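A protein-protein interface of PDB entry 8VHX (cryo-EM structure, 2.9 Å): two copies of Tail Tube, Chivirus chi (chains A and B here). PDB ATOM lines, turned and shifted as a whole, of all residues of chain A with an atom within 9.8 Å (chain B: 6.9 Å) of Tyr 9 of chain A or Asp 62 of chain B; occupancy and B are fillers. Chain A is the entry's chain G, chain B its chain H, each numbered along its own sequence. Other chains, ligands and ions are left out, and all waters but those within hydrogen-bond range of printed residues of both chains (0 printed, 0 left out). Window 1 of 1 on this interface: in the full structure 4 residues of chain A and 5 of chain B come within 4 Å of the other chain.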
ATOM      1  N   ASN A   2      -7.232 -15.132  36.346  1.00  0.00           N
ATOM      2  CA  ASN A   2      -6.627 -14.246  35.366  1.00  0.00           C
ATOM      3  C   ASN A   2      -7.367 -14.257  34.039  1.00  0.00           C
ATOM      4  O   ASN A   2      -6.927 -13.604  33.089  1.00  0.00           O
ATOM      5  CB  ASN A   2      -5.169 -14.641  35.154  1.00  0.00           C
ATOM      6  CG  ASN A   2      -4.998 -16.120  34.918  1.00  0.00           C
ATOM      7  OD1 ASN A   2      -5.850 -16.772  34.319  1.00  0.00           O
ATOM      8  ND2 ASN A   2      -3.908 -16.667  35.425  1.00  0.00           N
ATOM      9  N   ASP A   3      -8.481 -14.982  33.956  1.00  0.00           N
ATOM     10  CA  ASP A   3      -9.174 -15.152  32.687  1.00  0.00           C
ATOM     11  C   ASP A   3      -9.796 -13.858  32.185  1.00  0.00           C
ATOM     12  O   ASP A   3     -10.122 -13.760  30.999  1.00  0.00           O
ATOM     13  CB  ASP A   3     -10.248 -16.225  32.840  1.00  0.00           C
ATOM     14  CG  ASP A   3     -11.152 -15.975  34.029  1.00  0.00           C
ATOM     15  OD1 ASP A   3     -10.620 -15.759  35.139  1.00  0.00           O
ATOM     16  OD2 ASP A   3     -12.387 -15.991  33.855  1.00  0.00           O
ATOM     17  N   ASN A   4      -9.960 -12.869  33.059  1.00  0.00           N
ATOM     18  CA  ASN A   4     -10.589 -11.598  32.726  1.00  0.00           C
ATOM     19  C   ASN A   4      -9.643 -10.427  32.933  1.00  0.00           C
ATOM     20  O   ASN A   4     -10.076  -9.273  32.969  1.00  0.00           O
ATOM     21  CB  ASN A   4     -11.848 -11.438  33.563  1.00  0.00           C
ATOM     22  CG  ASN A   4     -11.601 -11.734  35.023  1.00  0.00           C
ATOM     23  OD1 ASN A   4     -10.484 -11.590  35.516  1.00  0.00           O
ATOM     24  ND2 ASN A   4     -12.625 -12.222  35.706  1.00  0.00           N
ATOM     25  N   TYR A   5      -8.359 -10.715  33.067  1.00  0.00           N
ATOM     26  CA  TYR A   5      -7.351  -9.687  33.232  1.00  0.00           C
ATOM     27  C   TYR A   5      -7.303  -8.784  32.011  1.00  0.00           C
ATOM     28  O   TYR A   5      -7.374  -9.249  30.871  1.00  0.00           O
ATOM     29  CB  TYR A   5      -6.016 -10.368  33.456  1.00  0.00           C
ATOM     30  CG  TYR A   5      -4.835  -9.490  33.699  1.00  0.00           C
ATOM     31  CD1 TYR A   5      -4.617  -8.919  34.935  1.00  0.00           C
ATOM     32  CD2 TYR A   5      -3.900  -9.284  32.715  1.00  0.00           C
ATOM     33  CE1 TYR A   5      -3.520  -8.138  35.156  1.00  0.00           C
ATOM     34  CE2 TYR A   5      -2.809  -8.511  32.934  1.00  0.00           C
ATOM     35  CZ  TYR A   5      -2.618  -7.941  34.150  1.00  0.00           C
ATOM     36  OH  TYR A   5      -1.511  -7.167  34.346  1.00  0.00           O
ATOM     37  N   GLN A   6      -7.188  -7.483  32.253  1.00  0.00           N
ATOM     38  CA  GLN A   6      -7.177  -6.493  31.183  1.00  0.00           C
ATOM     39  C   GLN A   6      -5.737  -6.114  30.875  1.00  0.00           C
ATOM     40  O   GLN A   6      -5.131  -5.298  31.572  1.00  0.00           O
ATOM     41  CB  GLN A   6      -7.999  -5.275  31.571  1.00  0.00           C
ATOM     42  CG  GLN A   6      -9.479  -5.532  31.628  1.00  0.00           C
ATOM     43  CD  GLN A   6     -10.052  -6.002  30.310  1.00  0.00           C
ATOM     44  OE1 GLN A   6     -10.857  -6.930  30.269  1.00  0.00           O
ATOM     45  NE2 GLN A   6      -9.644  -5.360  29.223  1.00  0.00           N
ATOM     46  N   ASN A   7      -5.196  -6.703  29.817  1.00  0.00           N
ATOM     47  CA  ASN A   7      -3.837  -6.401  29.408  1.00  0.00           C
ATOM     48  C   ASN A   7      -3.776  -5.005  28.802  1.00  0.00           C
ATOM     49  O   ASN A   7      -4.699  -4.567  28.114  1.00  0.00           O
ATOM     50  CB  ASN A   7      -3.361  -7.446  28.406  1.00  0.00           C
ATOM     51  CG  ASN A   7      -3.594  -8.854  28.877  1.00  0.00           C
ATOM     52  OD1 ASN A   7      -4.726  -9.321  28.928  1.00  0.00           O
ATOM     53  ND2 ASN A   7      -2.520  -9.553  29.193  1.00  0.00           N
ATOM     54  N   ASN A   8      -2.688  -4.293  29.084  1.00  0.00           N
ATOM     55  CA  ASN A   8      -2.479  -2.953  28.541  1.00  0.00           C
ATOM     56  C   ASN A   8      -1.753  -3.053  27.210  1.00  0.00           C
ATOM     57  O   ASN A   8      -0.532  -2.940  27.115  1.00  0.00           O
ATOM     58  CB  ASN A   8      -1.701  -2.086  29.510  1.00  0.00           C
ATOM     59  CG  ASN A   8      -1.426  -0.728  28.958  1.00  0.00           C
ATOM     60  OD1 ASN A   8      -2.322  -0.033  28.494  1.00  0.00           O
ATOM     61  ND2 ASN A   8      -0.177  -0.337  29.002  1.00  0.00           N
ATOM     62  N   TYR A   9      -2.529  -3.275  26.161  1.00  0.00           N
ATOM     63  CA  TYR A   9      -1.972  -3.290  24.823  1.00  0.00           C
ATOM     64  C   TYR A   9      -1.708  -1.870  24.359  1.00  0.00           C
ATOM     65  O   TYR A   9      -2.576  -1.001  24.464  1.00  0.00           O
ATOM     66  CB  TYR A   9      -2.917  -3.998  23.870  1.00  0.00           C
ATOM     67  CG  TYR A   9      -3.258  -5.397  24.292  1.00  0.00           C
ATOM     68  CD1 TYR A   9      -2.284  -6.247  24.767  1.00  0.00           C
ATOM     69  CD2 TYR A   9      -4.545  -5.878  24.192  1.00  0.00           C
ATOM     70  CE1 TYR A   9      -2.582  -7.513  25.146  1.00  0.00           C
ATOM     71  CE2 TYR A   9      -4.845  -7.149  24.570  1.00  0.00           C
ATOM     72  CZ  TYR A   9      -3.864  -7.964  25.041  1.00  0.00           C
ATOM     73  OH  TYR A   9      -4.191  -9.240  25.412  1.00  0.00           O
ATOM     74  N   VAL A  10      -0.505  -1.640  23.851  1.00  0.00           N
ATOM     75  CA  VAL A  10      -0.005  -0.309  23.550  1.00  0.00           C
ATOM     76  C   VAL A  10       0.369  -0.233  22.080  1.00  0.00           C
ATOM     77  O   VAL A  10       0.979  -1.156  21.535  1.00  0.00           O
ATOM     78  CB  VAL A  10       1.204   0.026  24.437  1.00  0.00           C
ATOM     79  CG1 VAL A  10       1.931   1.198  23.918  1.00  0.00           C
ATOM     80  CG2 VAL A  10       0.759   0.304  25.808  1.00  0.00           C
ATOM     81  N   VAL A  11      -0.005   0.869  21.445  1.00  0.00           N
ATOM     82  CA  VAL A  11       0.467   1.236  20.117  1.00  0.00           C
ATOM     83  C   VAL A  11       1.347   2.462  20.277  1.00  0.00           C
ATOM     84  O   VAL A  11       0.864   3.550  20.608  1.00  0.00           O
ATOM     85  CB  VAL A  11      -0.685   1.504  19.151  1.00  0.00           C
ATOM     86  CG1 VAL A  11      -0.165   2.072  17.886  1.00  0.00           C
ATOM     87  CG2 VAL A  11      -1.405   0.255  18.859  1.00  0.00           C
ATOM     88  N   GLY A  12       2.639   2.297  20.020  1.00  0.00           N
ATOM     89  CA  GLY A  12       3.602   3.301  20.406  1.00  0.00           C
ATOM     90  C   GLY A  12       3.545   4.534  19.537  1.00  0.00           C
ATOM     91  O   GLY A  12       3.710   4.450  18.309  1.00  0.00           O
ATOM     92  N   ASN A 223       0.256   7.823  23.195  1.00  0.00           N
ATOM     93  CA  ASN A 223      -0.214   6.562  22.664  1.00  0.00           C
ATOM     94  C   ASN A 223      -1.715   6.597  22.434  1.00  0.00           C
ATOM     95  O   ASN A 223      -2.476   6.781  23.393  1.00  0.00           O
ATOM     96  CB  ASN A 223       0.152   5.435  23.608  1.00  0.00           C
ATOM     97  CG  ASN A 223       1.622   5.169  23.634  1.00  0.00           C
ATOM     98  OD1 ASN A 223       2.342   5.518  22.707  1.00  0.00           O
ATOM     99  ND2 ASN A 223       2.093   4.588  24.712  1.00  0.00           N
ATOM    100  N   PRO A 224      -2.183   6.417  21.200  1.00  0.00           N
ATOM    101  CA  PRO A 224      -3.625   6.400  20.966  1.00  0.00           C
ATOM    102  C   PRO A 224      -4.292   5.199  21.577  1.00  0.00           C
ATOM    103  O   PRO A 224      -5.517   5.194  21.741  1.00  0.00           O
ATOM    104  CB  PRO A 224      -3.720   6.360  19.445  1.00  0.00           C
ATOM    105  CG  PRO A 224      -2.523   5.631  19.062  1.00  0.00           C
ATOM    106  CD  PRO A 224      -1.451   6.042  19.986  1.00  0.00           C
ATOM    107  N   VAL A 225      -3.515   4.176  21.908  1.00  0.00           N
ATOM    108  CA  VAL A 225      -4.018   2.943  22.487  1.00  0.00           C
ATOM    109  C   VAL A 225      -3.083   2.545  23.610  1.00  0.00           C
ATOM    110  O   VAL A 225      -1.864   2.502  23.425  1.00  0.00           O
ATOM    111  CB  VAL A 225      -4.108   1.827  21.440  1.00  0.00           C
ATOM    112  CG1 VAL A 225      -4.773   0.627  22.020  1.00  0.00           C
ATOM    113  CG2 VAL A 225      -4.854   2.325  20.262  1.00  0.00           C
ATOM    114  N   GLY A 226      -3.653   2.248  24.764  1.00  0.00           N
ATOM    115  CA  GLY A 226      -2.874   1.899  25.924  1.00  0.00           C
ATOM    116  C   GLY A 226      -2.400   3.112  26.691  1.00  0.00           C
ATOM    117  O   GLY A 226      -2.486   4.255  26.253  1.00  0.00           O
ATOM    118  N   LEU A 227      -1.891   2.835  27.881  1.00  0.00           N
ATOM    119  CA  LEU A 227      -1.490   3.886  28.790  1.00  0.00           C
ATOM    120  C   LEU A 227      -0.158   4.480  28.365  1.00  0.00           C
ATOM    121  O   LEU A 227       0.694   3.807  27.785  1.00  0.00           O
ATOM    122  CB  LEU A 227      -1.398   3.341  30.209  1.00  0.00           C
ATOM    123  CG  LEU A 227      -2.641   2.593  30.670  1.00  0.00           C
ATOM    124  CD1 LEU A 227      -2.434   2.083  32.057  1.00  0.00           C
ATOM    125  CD2 LEU A 227      -3.863   3.460  30.609  1.00  0.00           C
ATOM    126  N   ASN A 228       0.015   5.758  28.670  1.00  0.00           N
ATOM    127  CA  ASN A 228       1.202   6.486  28.275  1.00  0.00           C
ATOM    128  C   ASN A 228       2.324   6.281  29.278  1.00  0.00           C
ATOM    129  O   ASN A 228       2.092   6.173  30.482  1.00  0.00           O
ATOM    130  CB  ASN A 228       0.884   7.968  28.147  1.00  0.00           C
ATOM    131  CG  ASN A 228      -0.184   8.244  27.133  1.00  0.00           C
ATOM    132  OD1 ASN A 228       0.053   8.186  25.931  1.00  0.00           O
ATOM    133  ND2 ASN A 228      -1.380   8.520  27.609  1.00  0.00           N
ATOM    134  N   LYS A 229       3.546   6.220  28.765  1.00  0.00           N
ATOM    135  CA  LYS A 229       4.741   6.106  29.581  1.00  0.00           C
ATOM    136  C   LYS A 229       5.824   6.978  28.983  1.00  0.00           C
ATOM    137  O   LYS A 229       6.032   6.967  27.768  1.00  0.00           O
ATOM    138  CB  LYS A 229       5.218   4.667  29.667  1.00  0.00           C
ATOM    139  CG  LYS A 229       4.273   3.816  30.413  1.00  0.00           C
ATOM    140  CD  LYS A 229       4.740   2.407  30.501  1.00  0.00           C
ATOM    141  CE  LYS A 229       3.817   1.630  31.363  1.00  0.00           C
ATOM    142  NZ  LYS A 229       2.449   1.716  30.850  1.00  0.00           N
ATOM    143  N   ASP B  50      -5.723  -5.835  14.927  1.00  0.00           N
ATOM    144  CA  ASP B  50      -6.383  -6.772  15.815  1.00  0.00           C
ATOM    145  C   ASP B  50      -5.358  -7.534  16.635  1.00  0.00           C
ATOM    146  O   ASP B  50      -4.344  -7.997  16.108  1.00  0.00           O
ATOM    147  CB  ASP B  50      -7.240  -7.749  15.022  1.00  0.00           C
ATOM    148  CG  ASP B  50      -8.307  -7.060  14.210  1.00  0.00           C
ATOM    149  OD1 ASP B  50      -8.643  -5.903  14.528  1.00  0.00           O
ATOM    150  OD2 ASP B  50      -8.807  -7.672  13.247  1.00  0.00           O
ATOM    151  N   HIS B  51      -5.628  -7.657  17.927  1.00  0.00           N
ATOM    152  CA  HIS B  51      -4.811  -8.438  18.836  1.00  0.00           C
ATOM    153  C   HIS B  51      -5.635  -9.596  19.371  1.00  0.00           C
ATOM    154  O   HIS B  51      -6.802  -9.425  19.726  1.00  0.00           O
ATOM    155  CB  HIS B  51      -4.299  -7.579  19.988  1.00  0.00           C
ATOM    156  CG  HIS B  51      -3.237  -8.233  20.806  1.00  0.00           C
ATOM    157  ND1 HIS B  51      -3.514  -9.199  21.742  1.00  0.00           N
ATOM    158  CD2 HIS B  51      -1.897  -8.055  20.837  1.00  0.00           C
ATOM    159  CE1 HIS B  51      -2.391  -9.596  22.310  1.00  0.00           C
ATOM    160  NE2 HIS B  51      -1.394  -8.918  21.777  1.00  0.00           N
ATOM    161  N   TYR B  52      -5.026 -10.771  19.420  1.00  0.00           N
ATOM    162  CA  TYR B  52      -5.700 -11.994  19.812  1.00  0.00           C
ATOM    163  C   TYR B  52      -5.068 -12.561  21.070  1.00  0.00           C
ATOM    164  O   TYR B  52      -3.847 -12.518  21.237  1.00  0.00           O
ATOM    165  CB  TYR B  52      -5.633 -13.015  18.704  1.00  0.00           C
ATOM    166  CG  TYR B  52      -6.197 -12.537  17.400  1.00  0.00           C
ATOM    167  CD1 TYR B  52      -7.531 -12.710  17.101  1.00  0.00           C
ATOM    168  CD2 TYR B  52      -5.401 -11.915  16.465  1.00  0.00           C
ATOM    169  CE1 TYR B  52      -8.051 -12.284  15.921  1.00  0.00           C
ATOM    170  CE2 TYR B  52      -5.918 -11.485  15.278  1.00  0.00           C
ATOM    171  CZ  TYR B  52      -7.246 -11.672  15.011  1.00  0.00           C
ATOM    172  OH  TYR B  52      -7.785 -11.245  13.825  1.00  0.00           O
ATOM    173  N   SER B  53      -5.904 -13.100  21.947  1.00  0.00           N
ATOM    174  CA  SER B  53      -5.416 -13.646  23.200  1.00  0.00           C
ATOM    175  C   SER B  53      -4.612 -14.903  22.943  1.00  0.00           C
ATOM    176  O   SER B  53      -5.100 -15.854  22.327  1.00  0.00           O
ATOM    177  CB  SER B  53      -6.576 -13.946  24.138  1.00  0.00           C
ATOM    178  OG  SER B  53      -6.093 -14.393  25.388  1.00  0.00           O
ATOM    179  N   SER B  54      -3.370 -14.892  23.401  1.00  0.00           N
ATOM    180  CA  SER B  54      -2.505 -16.054  23.322  1.00  0.00           C
ATOM    181  C   SER B  54      -2.502 -16.872  24.597  1.00  0.00           C
ATOM    182  O   SER B  54      -1.828 -17.902  24.652  1.00  0.00           O
ATOM    183  CB  SER B  54      -1.078 -15.625  23.009  1.00  0.00           C
ATOM    184  OG  SER B  54      -1.032 -14.870  21.815  1.00  0.00           O
ATOM    185  N   ARG B  59      -7.999 -18.388  19.036  1.00  0.00           N
ATOM    186  CA  ARG B  59      -7.649 -17.103  18.452  1.00  0.00           C
ATOM    187  C   ARG B  59      -8.666 -16.052  18.893  1.00  0.00           C
ATOM    188  O   ARG B  59      -9.230 -15.308  18.100  1.00  0.00           O
ATOM    189  CB  ARG B  59      -7.527 -17.186  16.935  1.00  0.00           C
ATOM    190  CG  ARG B  59      -7.002 -15.914  16.345  1.00  0.00           C
ATOM    191  CD  ARG B  59      -6.465 -16.110  14.966  1.00  0.00           C
ATOM    192  NE  ARG B  59      -5.182 -16.787  15.021  1.00  0.00           N
ATOM    193  CZ  ARG B  59      -4.488 -17.144  13.955  1.00  0.00           C
ATOM    194  NH1 ARG B  59      -3.329 -17.758  14.099  1.00  0.00           N
ATOM    195  NH2 ARG B  59      -4.953 -16.882  12.747  1.00  0.00           N
ATOM    196  N   VAL B  60      -8.921 -16.008  20.195  1.00  0.00           N
ATOM    197  CA  VAL B  60      -9.864 -15.058  20.766  1.00  0.00           C
ATOM    198  C   VAL B  60      -9.330 -13.644  20.604  1.00  0.00           C
ATOM    199  O   VAL B  60      -8.280 -13.293  21.150  1.00  0.00           O
ATOM    200  CB  VAL B  60     -10.119 -15.378  22.239  1.00  0.00           C
ATOM    201  CG1 VAL B  60     -10.730 -14.212  22.921  1.00  0.00           C
ATOM    202  CG2 VAL B  60     -11.016 -16.568  22.362  1.00  0.00           C
ATOM    203  N   MET B  61     -10.062 -12.822  19.861  1.00  0.00           N
ATOM    204  CA  MET B  61      -9.761 -11.403  19.789  1.00  0.00           C
ATOM    205  C   MET B  61     -10.081 -10.731  21.112  1.00  0.00           C
ATOM    206  O   MET B  61     -11.132 -10.972  21.711  1.00  0.00           O
ATOM    207  CB  MET B  61     -10.554 -10.751  18.663  1.00  0.00           C
ATOM    208  CG  MET B  61     -10.167  -9.329  18.390  1.00  0.00           C
ATOM    209  SD  MET B  61     -11.352  -8.471  17.362  1.00  0.00           S
ATOM    210  CE  MET B  61     -11.115  -9.386  15.856  1.00  0.00           C
ATOM    211  N   ASP B  62      -9.167  -9.885  21.564  1.00  0.00           N
ATOM    212  CA  ASP B  62      -9.334  -9.143  22.795  1.00  0.00           C
ATOM    213  C   ASP B  62      -9.145  -7.651  22.620  1.00  0.00           C
ATOM    214  O   ASP B  62      -9.507  -6.892  23.524  1.00  0.00           O
ATOM    215  CB  ASP B  62      -8.348  -9.649  23.847  1.00  0.00           C
ATOM    216  CG  ASP B  62      -6.926  -9.470  23.424  1.00  0.00           C
ATOM    217  OD1 ASP B  62      -6.709  -9.051  22.274  1.00  0.00           O
ATOM    218  OD2 ASP B  62      -6.024  -9.771  24.225  1.00  0.00           O
ATOM    219  N   ALA B  63      -8.597  -7.209  21.495  1.00  0.00           N
ATOM    220  CA  ALA B  63      -8.409  -5.800  21.219  1.00  0.00           C
ATOM    221  C   ALA B  63      -8.408  -5.593  19.717  1.00  0.00           C
ATOM    222  O   ALA B  63      -7.888  -6.415  18.963  1.00  0.00           O
ATOM    223  CB  ALA B  63      -7.115  -5.284  21.828  1.00  0.00           C
ATOM    224  N   SER B  64      -8.994  -4.480  19.294  1.00  0.00           N
ATOM    225  CA  SER B  64      -9.068  -4.137  17.883  1.00  0.00           C
ATOM    226  C   SER B  64      -9.237  -2.635  17.789  1.00  0.00           C
ATOM    227  O   SER B  64     -10.184  -2.087  18.358  1.00  0.00           O
ATOM    228  CB  SER B  64     -10.224  -4.852  17.203  1.00  0.00           C
ATOM    229  OG  SER B  64     -10.342  -4.474  15.849  1.00  0.00           O
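Of the 18 printed residues of chain A, 1 touches a printed residue of chain B. Printed residues of chain A that touch a printed residue of chain B: Tyr 9. Printed residues of chain B that touch a printed residue of chain A: His 51, Asp 62 and Ala 63. Hydrophobic or aromatic side chains of chain B within 4 Å of the printed part of chain A: His 51 and Ala 63. Among the printed residues, no Asp or Glu carboxylate lies within 4 Å of a Lys or Arg side-chain nitrogen of the other chain.
No position is printed for both chains.
CZ of Tyr 9 of chain A touches CE1 of His 51 of chain B (3.5 Å). CB of Ala 63 of chain B touches CD2 of Tyr 9 of chain A, 3.5 Å away.
Tyr 9 of chain A touches just these residues of chain B: His 51 (3.5 Å), Asp 62 (2.2 Å) and Ala 63 (3.5 Å). Of the printed residues of chain A, His 51 of chain B touches Tyr 9 (3.5 Å). Of chain A, only Tyr 9 (3.5 Å) comes within 4 Å of Ala 63 of chain B. Tyr 52 of chain B touches none of the printed residues of chain A. Leu 227 of chain A touches none of the printed residues of chain B. The nearest residue of chain B that does not touch Tyr 9 of chain A is Ser 53 of chain B (5.1 Å).
The side-chain carboxylate (OD2) of Asp 62 of chain B lies close to the side-chain hydroxyl (OH) of Tyr 9 of chain A, 2.2 Å away.
N of Gly 226 of chain A sits close to O of Tyr 9 of chain A (3.4 Å). The backbone carbonyl oxygen (O) of His 51 of chain B sits at hydrogen-bond distance from the backbone NH (N) of Asp 62 of chain B, 3.0 Å away. The backbone carbonyl oxygen of Ala 63 of chain B lies within hydrogen-bond range of the backbone NH of His 51 of chain B, at 2.8 Å.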
